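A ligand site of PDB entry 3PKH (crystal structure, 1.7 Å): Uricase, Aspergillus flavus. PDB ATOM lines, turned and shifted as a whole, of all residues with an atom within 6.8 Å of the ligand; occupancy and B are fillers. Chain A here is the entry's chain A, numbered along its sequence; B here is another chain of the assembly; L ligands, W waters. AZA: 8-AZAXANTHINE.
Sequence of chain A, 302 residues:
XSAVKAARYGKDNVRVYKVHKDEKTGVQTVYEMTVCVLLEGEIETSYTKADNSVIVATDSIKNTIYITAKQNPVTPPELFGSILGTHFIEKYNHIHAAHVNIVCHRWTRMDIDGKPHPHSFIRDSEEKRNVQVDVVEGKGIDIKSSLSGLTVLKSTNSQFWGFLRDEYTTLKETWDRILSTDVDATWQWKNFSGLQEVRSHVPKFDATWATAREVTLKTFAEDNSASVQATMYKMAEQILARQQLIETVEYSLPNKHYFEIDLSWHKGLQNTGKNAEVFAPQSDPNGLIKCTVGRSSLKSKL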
ATOM      1  N   SER A 158      30.634  35.073 -26.731  1.00  0.00           N
ATOM      2  CA  SER A 158      29.943  33.885 -26.292  1.00  0.00           C
ATOM      3  C   SER A 158      29.883  32.954 -27.491  1.00  0.00           C
ATOM      4  O   SER A 158      29.593  33.384 -28.616  1.00  0.00           O
ATOM      5  CB  SER A 158      28.517  34.239 -25.830  1.00  0.00           C
ATOM      6  OG  SER A 158      27.783  33.047 -25.552  1.00  0.00           O
ATOM      7  N   GLN A 159      30.160  31.664 -27.251  1.00  0.00           N
ATOM      8  CA  GLN A 159      30.162  30.624 -28.259  1.00  0.00           C
ATOM      9  C   GLN A 159      29.370  29.439 -27.765  1.00  0.00           C
ATOM     10  O   GLN A 159      29.154  29.270 -26.556  1.00  0.00           O
ATOM     11  CB  GLN A 159      31.617  30.156 -28.551  1.00  0.00           C
ATOM     12  CG  GLN A 159      32.598  31.315 -28.744  1.00  0.00           C
ATOM     13  CD  GLN A 159      33.988  30.857 -29.153  1.00  0.00           C
ATOM     14  OE1 GLN A 159      34.265  29.674 -29.251  1.00  0.00           O
ATOM     15  NE2 GLN A 159      34.867  31.823 -29.403  1.00  0.00           N
ATOM     16  N   PHE A 160      28.921  28.609 -28.695  1.00  0.00           N
ATOM     17  CA  PHE A 160      28.323  27.334 -28.336  1.00  0.00           C
ATOM     18  C   PHE A 160      28.425  26.345 -29.502  1.00  0.00           C
ATOM     19  O   PHE A 160      27.629  26.361 -30.423  1.00  0.00           O
ATOM     20  CB  PHE A 160      26.869  27.491 -27.791  1.00  0.00           C
ATOM     21  CG  PHE A 160      26.343  26.234 -27.166  1.00  0.00           C
ATOM     22  CD1 PHE A 160      26.914  25.739 -25.999  1.00  0.00           C
ATOM     23  CD2 PHE A 160      25.277  25.543 -27.749  1.00  0.00           C
ATOM     24  CE1 PHE A 160      26.450  24.561 -25.408  1.00  0.00           C
ATOM     25  CE2 PHE A 160      24.788  24.365 -27.156  1.00  0.00           C
ATOM     26  CZ  PHE A 160      25.394  23.854 -26.004  1.00  0.00           C
ATOM     27  N   PHE A 163      28.396  20.447 -29.184  1.00  0.00           N
ATOM     28  CA  PHE A 163      27.375  19.668 -28.470  1.00  0.00           C
ATOM     29  C   PHE A 163      26.916  18.403 -29.235  1.00  0.00           C
ATOM     30  O   PHE A 163      27.196  18.250 -30.437  1.00  0.00           O
ATOM     31  CB  PHE A 163      26.149  20.562 -28.130  1.00  0.00           C
ATOM     32  CG  PHE A 163      25.641  21.361 -29.300  1.00  0.00           C
ATOM     33  CD1 PHE A 163      26.165  22.609 -29.570  1.00  0.00           C
ATOM     34  CD2 PHE A 163      24.611  20.858 -30.118  1.00  0.00           C
ATOM     35  CE1 PHE A 163      25.714  23.377 -30.651  1.00  0.00           C
ATOM     36  CE2 PHE A 163      24.139  21.623 -31.205  1.00  0.00           C
ATOM     37  CZ  PHE A 163      24.699  22.867 -31.473  1.00  0.00           C
ATOM     38  N   LEU A 171      19.783  22.701 -33.966  1.00  0.00           N
ATOM     39  CA  LEU A 171      20.586  23.877 -33.581  1.00  0.00           C
ATOM     40  C   LEU A 171      21.945  23.925 -34.322  1.00  0.00           C
ATOM     41  O   LEU A 171      22.705  22.952 -34.299  1.00  0.00           O
ATOM     42  CB  LEU A 171      20.818  23.854 -32.066  1.00  0.00           C
ATOM     43  CG  LEU A 171      21.597  25.062 -31.498  1.00  0.00           C
ATOM     44  CD1 LEU A 171      20.808  26.353 -31.651  1.00  0.00           C
ATOM     45  CD2 LEU A 171      21.951  24.825 -30.023  1.00  0.00           C
ATOM     46  N   ARG A 177      27.709  34.655 -30.444  1.00  0.00           N
ATOM     47  CA  ARG A 177      26.268  34.850 -30.171  1.00  0.00           C
ATOM     48  C   ARG A 177      26.084  35.825 -29.038  1.00  0.00           C
ATOM     49  O   ARG A 177      27.040  36.219 -28.357  1.00  0.00           O
ATOM     50  CB  ARG A 177      25.580  33.515 -29.829  1.00  0.00           C
ATOM     51  CG  ARG A 177      26.090  32.908 -28.534  1.00  0.00           C
ATOM     52  CD  ARG A 177      25.394  31.601 -28.161  1.00  0.00           C
ATOM     53  NE  ARG A 177      25.806  31.207 -26.806  1.00  0.00           N
ATOM     54  CZ  ARG A 177      25.270  30.224 -26.082  1.00  0.00           C
ATOM     55  NH1 ARG A 177      24.306  29.429 -26.588  1.00  0.00           N
ATOM     56  NH2 ARG A 177      25.748  29.992 -24.862  1.00  0.00           N
ATOM     57  N   LEU A 179      24.663  36.599 -25.360  1.00  0.00           N
ATOM     58  CA  LEU A 179      24.363  35.848 -24.120  1.00  0.00           C
ATOM     59  C   LEU A 179      23.725  36.798 -23.107  1.00  0.00           C
ATOM     60  O   LEU A 179      24.299  37.835 -22.764  1.00  0.00           O
ATOM     61  CB  LEU A 179      25.651  35.259 -23.534  1.00  0.00           C
ATOM     62  CG  LEU A 179      25.563  34.480 -22.234  1.00  0.00           C
ATOM     63  CD1 LEU A 179      24.607  33.307 -22.366  1.00  0.00           C
ATOM     64  CD2 LEU A 179      26.984  33.971 -21.851  1.00  0.00           C
ATOM     65  N   SER A 225      33.044  32.890 -23.421  1.00  0.00           N
ATOM     66  CA  SER A 225      32.245  31.823 -22.853  1.00  0.00           C
ATOM     67  C   SER A 225      32.028  30.652 -23.813  1.00  0.00           C
ATOM     68  O   SER A 225      31.572  30.815 -24.952  1.00  0.00           O
ATOM     69  CB  SER A 225      30.901  32.409 -22.380  1.00  0.00           C
ATOM     70  OG  SER A 225      30.026  31.360 -22.015  1.00  0.00           O
ATOM     71  N   ALA A 226      32.337  29.466 -23.321  1.00  0.00           N
ATOM     72  CA  ALA A 226      32.169  28.266 -24.095  1.00  0.00           C
ATOM     73  C   ALA A 226      30.756  27.696 -23.961  1.00  0.00           C
ATOM     74  O   ALA A 226      30.329  26.851 -24.765  1.00  0.00           O
ATOM     75  CB  ALA A 226      33.218  27.217 -23.626  1.00  0.00           C
ATOM     76  N   SER A 227      30.035  28.159 -22.934  1.00  0.00           N
ATOM     77  CA  SER A 227      28.657  27.739 -22.624  1.00  0.00           C
ATOM     78  C   SER A 227      28.280  28.447 -21.332  1.00  0.00           C
ATOM     79  O   SER A 227      29.143  28.952 -20.615  1.00  0.00           O
ATOM     80  CB  SER A 227      28.506  26.209 -22.394  1.00  0.00           C
ATOM     81  OG  SER A 227      29.277  25.755 -21.256  1.00  0.00           O
ATOM     82  N   VAL A 228      26.984  28.474 -21.020  1.00  0.00           N
ATOM     83  CA  VAL A 228      26.571  29.029 -19.734  1.00  0.00           C
ATOM     84  C   VAL A 228      27.182  28.165 -18.616  1.00  0.00           C
ATOM     85  O   VAL A 228      27.656  28.688 -17.597  1.00  0.00           O
ATOM     86  CB  VAL A 228      25.012  29.001 -19.658  1.00  0.00           C
ATOM     87  CG1 VAL A 228      24.515  29.352 -18.271  1.00  0.00           C
ATOM     88  CG2 VAL A 228      24.464  29.983 -20.701  1.00  0.00           C
ATOM     89  N   GLN A 229      27.186  26.852 -18.832  1.00  0.00           N
ATOM     90  CA  GLN A 229      27.716  25.852 -17.867  1.00  0.00           C
ATOM     91  C   GLN A 229      29.164  26.211 -17.482  1.00  0.00           C
ATOM     92  O   GLN A 229      29.515  26.289 -16.274  1.00  0.00           O
ATOM     93  CB  GLN A 229      27.678  24.452 -18.491  1.00  0.00           C
ATOM     94  CG  GLN A 229      26.293  23.774 -18.587  1.00  0.00           C
ATOM     95  CD  GLN A 229      25.499  24.107 -19.842  1.00  0.00           C
ATOM     96  OE1 GLN A 229      25.690  25.162 -20.473  1.00  0.00           O
ATOM     97  NE2 GLN A 229      24.565  23.219 -20.186  1.00  0.00           N
ATOM     98  N   ASN A 255      18.819  31.042 -19.980  1.00  0.00           N
ATOM     99  CA  ASN A 255      19.509  31.470 -21.171  1.00  0.00           C
ATOM    100  C   ASN A 255      18.438  32.180 -21.994  1.00  0.00           C
ATOM    101  O   ASN A 255      17.590  31.510 -22.547  1.00  0.00           O
ATOM    102  CB  ASN A 255      20.112  30.240 -21.865  1.00  0.00           C
ATOM    103  CG  ASN A 255      21.012  30.607 -23.028  1.00  0.00           C
ATOM    104  OD1 ASN A 255      21.238  31.790 -23.327  1.00  0.00           O
ATOM    105  ND2 ASN A 255      21.513  29.587 -23.730  1.00  0.00           N
ATOM    106  N   HIS A 257      17.089  33.859 -24.989  1.00  0.00           N
ATOM    107  CA  HIS A 257      17.570  33.787 -26.372  1.00  0.00           C
ATOM    108  C   HIS A 257      17.250  35.020 -27.204  1.00  0.00           C
ATOM    109  O   HIS A 257      16.168  35.577 -27.107  1.00  0.00           O
ATOM    110  CB  HIS A 257      17.014  32.538 -27.063  1.00  0.00           C
ATOM    111  CG  HIS A 257      17.231  31.272 -26.298  1.00  0.00           C
ATOM    112  ND1 HIS A 257      18.481  30.724 -26.103  1.00  0.00           N
ATOM    113  CD2 HIS A 257      16.356  30.454 -25.654  1.00  0.00           C
ATOM    114  CE1 HIS A 257      18.368  29.608 -25.409  1.00  0.00           C
ATOM    115  NE2 HIS A 257      17.090  29.431 -25.109  1.00  0.00           N
ATOM    116  N   GLY A 287      16.378  28.444 -22.074  1.00  0.00           N
ATOM    117  CA  GLY A 287      17.215  27.461 -21.386  1.00  0.00           C
ATOM    118  C   GLY A 287      17.246  27.776 -19.897  1.00  0.00           C
ATOM    119  O   GLY A 287      17.046  28.918 -19.462  1.00  0.00           O
ATOM    120  N   ILE A 289      19.801  26.619 -16.622  1.00  0.00           N
ATOM    121  CA  ILE A 289      21.017  25.860 -16.318  1.00  0.00           C
ATOM    122  C   ILE A 289      21.320  26.056 -14.847  1.00  0.00           C
ATOM    123  O   ILE A 289      21.381  27.189 -14.388  1.00  0.00           O
ATOM    124  CB  ILE A 289      22.230  26.413 -17.135  1.00  0.00           C
ATOM    125  CG1 ILE A 289      21.855  26.705 -18.606  1.00  0.00           C
ATOM    126  CG2 ILE A 289      23.447  25.425 -16.998  1.00  0.00           C
ATOM    127  CD1 ILE A 289      21.386  25.554 -19.365  1.00  0.00           C
ATOM    128  N   TYR B   9      20.043  20.760 -16.059  1.00  0.00           N
ATOM    129  CA  TYR B   9      19.894  21.810 -17.053  1.00  0.00           C
ATOM    130  C   TYR B   9      18.830  21.330 -18.039  1.00  0.00           C
ATOM    131  O   TYR B   9      18.567  20.130 -18.143  1.00  0.00           O
ATOM    132  CB  TYR B   9      21.243  22.104 -17.762  1.00  0.00           C
ATOM    133  CG  TYR B   9      21.471  21.129 -18.869  1.00  0.00           C
ATOM    134  CD1 TYR B   9      21.817  19.798 -18.588  1.00  0.00           C
ATOM    135  CD2 TYR B   9      21.213  21.479 -20.200  1.00  0.00           C
ATOM    136  CE1 TYR B   9      21.945  18.859 -19.608  1.00  0.00           C
ATOM    137  CE2 TYR B   9      21.337  20.548 -21.224  1.00  0.00           C
ATOM    138  CZ  TYR B   9      21.703  19.236 -20.910  1.00  0.00           C
ATOM    139  OH  TYR B   9      21.810  18.311 -21.908  1.00  0.00           O
ATOM    140  N   GLY B  10      18.233  22.269 -18.764  1.00  0.00           N
ATOM    141  CA  GLY B  10      17.217  21.921 -19.745  1.00  0.00           C
ATOM    142  C   GLY B  10      16.465  23.127 -20.269  1.00  0.00           C
ATOM    143  O   GLY B  10      17.016  24.207 -20.371  1.00  0.00           O
ATOM    144  N   LYS B  11      15.200  22.926 -20.623  1.00  0.00           N
ATOM    145  CA  LYS B  11      14.400  23.996 -21.266  1.00  0.00           C
ATOM    146  C   LYS B  11      13.161  24.257 -20.421  1.00  0.00           C
ATOM    147  O   LYS B  11      12.494  23.303 -20.002  1.00  0.00           O
ATOM    148  CB  LYS B  11      13.961  23.568 -22.676  1.00  0.00           C
ATOM    149  CG  LYS B  11      13.588  24.747 -23.594  1.00  0.00           C
ATOM    150  CD  LYS B  11      14.841  25.582 -23.869  1.00  0.00           C
ATOM    151  CE  LYS B  11      15.035  25.956 -25.318  1.00  0.00           C
ATOM    152  NZ  LYS B  11      16.407  26.535 -25.571  1.00  0.00           N
ATOM    153  N   ASN B  52      31.495  20.251 -24.310  1.00  0.00           N
ATOM    154  CA  ASN B  52      30.083  20.248 -24.738  1.00  0.00           C
ATOM    155  C   ASN B  52      29.580  18.914 -25.320  1.00  0.00           C
ATOM    156  O   ASN B  52      28.395  18.763 -25.600  1.00  0.00           O
ATOM    157  CB  ASN B  52      29.778  21.431 -25.669  1.00  0.00           C
ATOM    158  CG  ASN B  52      29.937  22.774 -24.970  1.00  0.00           C
ATOM    159  OD1 ASN B  52      29.829  22.854 -23.747  1.00  0.00           O
ATOM    160  ND2 ASN B  52      30.187  23.830 -25.741  1.00  0.00           N
ATOM    161  N   ILE B  55      26.560  17.459 -23.742  1.00  0.00           N
ATOM    162  CA  ILE B  55      25.330  18.245 -23.665  1.00  0.00           C
ATOM    163  C   ILE B  55      24.349  17.916 -24.777  1.00  0.00           C
ATOM    164  O   ILE B  55      24.661  18.075 -25.961  1.00  0.00           O
ATOM    165  CB  ILE B  55      25.609  19.764 -23.688  1.00  0.00           C
ATOM    166  CG1 ILE B  55      26.479  20.170 -22.498  1.00  0.00           C
ATOM    167  CG2 ILE B  55      24.256  20.565 -23.647  1.00  0.00           C
ATOM    168  CD1 ILE B  55      26.931  21.624 -22.572  1.00  0.00           C
ATOM    169  N   VAL B  56      23.167  17.449 -24.382  1.00  0.00           N
ATOM    170  CA  VAL B  56      21.998  17.399 -25.264  1.00  0.00           C
ATOM    171  C   VAL B  56      21.525  18.863 -25.269  1.00  0.00           C
ATOM    172  O   VAL B  56      21.110  19.358 -24.208  1.00  0.00           O
ATOM    173  CB  VAL B  56      20.923  16.425 -24.737  1.00  0.00           C
ATOM    174  CG1 VAL B  56      19.655  16.461 -25.621  1.00  0.00           C
ATOM    175  CG2 VAL B  56      21.482  14.984 -24.667  1.00  0.00           C
ATOM    176  N   ALA B  57      21.607  19.552 -26.410  1.00  0.00           N
ATOM    177  CA  ALA B  57      21.278  20.993 -26.435  1.00  0.00           C
ATOM    178  C   ALA B  57      19.852  21.228 -25.936  1.00  0.00           C
ATOM    179  O   ALA B  57      18.958  20.413 -26.173  1.00  0.00           O
ATOM    180  CB  ALA B  57      21.454  21.566 -27.837  1.00  0.00           C
ATOM    181  N   THR B  58      19.664  22.348 -25.227  1.00  0.00           N
ATOM    182  CA  THR B  58      18.344  22.632 -24.678  1.00  0.00           C
ATOM    183  C   THR B  58      17.378  22.848 -25.840  1.00  0.00           C
ATOM    184  O   THR B  58      16.206  22.485 -25.734  1.00  0.00           O
ATOM    185  CB  THR B  58      18.314  23.843 -23.726  1.00  0.00           C
ATOM    186  OG1 THR B  58      18.592  25.042 -24.456  1.00  0.00           O
ATOM    187  CG2 THR B  58      19.370  23.675 -22.588  1.00  0.00           C
ATOM    188  N   ASP B  59      17.887  23.389 -26.957  1.00  0.00           N
ATOM    189  CA  ASP B  59      17.090  23.491 -28.185  1.00  0.00           C
ATOM    190  C   ASP B  59      16.574  22.125 -28.656  1.00  0.00           C
ATOM    191  O   ASP B  59      15.446  22.000 -29.098  1.00  0.00           O
ATOM    192  CB  ASP B  59      17.882  24.185 -29.305  1.00  0.00           C
ATOM    193  CG  ASP B  59      17.020  24.526 -30.506  1.00  0.00           C
ATOM    194  OD1 ASP B  59      16.312  25.557 -30.456  1.00  0.00           O
ATOM    195  OD2 ASP B  59      17.025  23.769 -31.495  1.00  0.00           O
ATOM    196  N   SER B  60      17.413  21.087 -28.557  1.00  0.00           N
ATOM    197  CA  SER B  60      16.988  19.702 -28.865  1.00  0.00           C
ATOM    198  C   SER B  60      15.943  19.159 -27.905  1.00  0.00           C
ATOM    199  O   SER B  60      15.060  18.410 -28.301  1.00  0.00           O
ATOM    200  CB  SER B  60      18.225  18.769 -28.936  1.00  0.00           C
ATOM    201  OG  SER B  60      19.154  19.374 -29.813  1.00  0.00           O
HETATM  202  N1  AZA L   1      24.172  25.798 -22.902  1.00  0.00           N
HETATM  203  C2  AZA L   1      24.335  26.949 -23.605  1.00  0.00           C
HETATM  204  O2  AZA L   1      25.141  27.784 -23.169  1.00  0.00           O
HETATM  205  N3  AZA L   1      23.619  27.217 -24.761  1.00  0.00           N
HETATM  206  C4  AZA L   1      22.791  26.265 -25.202  1.00  0.00           C
HETATM  207  C5  AZA L   1      22.577  25.025 -24.513  1.00  0.00           C
HETATM  208  C6  AZA L   1      23.342  24.821 -23.276  1.00  0.00           C
HETATM  209  O6  AZA L   1      23.178  23.777 -22.628  1.00  0.00           O
HETATM  210  N7  AZA L   1      21.666  24.247 -25.190  1.00  0.00           N
HETATM  211  N8  AZA L   1      21.339  25.063 -26.282  1.00  0.00           N
HETATM  212  N9  AZA L   1      21.995  26.312 -26.328  1.00  0.00           N
HETATM  213  O   HOH W   1      20.038  27.134 -23.281  1.00  0.00           O
HETATM  214  O   HOH W   2      21.380  28.330 -27.991  1.00  0.00           O
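NH2 of Arg 177 sits at hydrogen-bond distance from O2 of the ligand (2.8 Å). The side-chain amide nitrogen (NE2) of Gln 229 sits at hydrogen-bond distance from an oxygen (O6) of the ligand (2.9 Å). N3 of the ligand sits close to ND2 of Asn 255, 3.3 Å away. N7 of the ligand lies within hydrogen-bond range of N of Thr 58 of chain B, at 2.8 Å. The side-chain hydroxyl of Thr 58 of chain B lies within hydrogen-bond range of a nitrogen (N7) of the ligand (3.3 Å). N of Val 228 is in hydrogen-bond range of O2 of the ligand (2.9 Å).
OG1 of Thr 58 of chain B lies within hydrogen-bond range of NZ of Lys 11 of chain B, at 2.9 Å. O of Ser 158 is in hydrogen-bond range of N of Arg 177 (2.9 Å). A ring nitrogen (NE2) of His 257 sits at hydrogen-bond distance from the backbone carbonyl oxygen (O) of Asn 255, 3.3 Å away. The backbone carbonyl oxygen (O) of Ser 227 lies within hydrogen-bond range of the side-chain hydroxyl (OG) of Ser 225 (2.9 Å). The side-chain hydroxyl of Tyr 9 of chain B is in hydrogen-bond range of the backbone carbonyl oxygen of Val 56 of chain B, 2.6 Å away. N of Asn 255 lies within hydrogen-bond range of O of Gly 287 (2.8 Å). N of Gln 229 sits close to OG of Ser 227 (3.4 Å).
CE2 of Phe 160 touches C4 of the ligand, at 3.4 Å. Leu 171 touches the ligand. Ser 227 touches the ligand (CA to O2, 3.6 Å). CD2 of Tyr 9 of chain B touches O6 of the ligand (3.9 Å). Ile 55 of chain B touches the ligand. CA of Ala 57 of chain B touches N7 of the ligand, at 3.5 Å. N of Asp 59 of chain B touches N8 of the ligand, 3.9 Å away. Within 4 Å of the ligand: Phe 160, Leu 171, Arg 177, Ser 227, Val 228, Gln 229, Asn 255, Tyr 9 of chain B, Ile 55 of chain B, Ala 57 of chain B, Thr 58 of chain B and Asp 59 of chain B.
Water W2 lies within hydrogen-bond range of a nitrogen (N9) of the ligand (2.7 Å) and the guanidinium group of Arg 177 (3.4 Å). Water W1 lies within hydrogen-bond range of OG1 of Thr 58 of chain B (2.8 Å) and ND2 of Asn 255 (2.9 Å).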
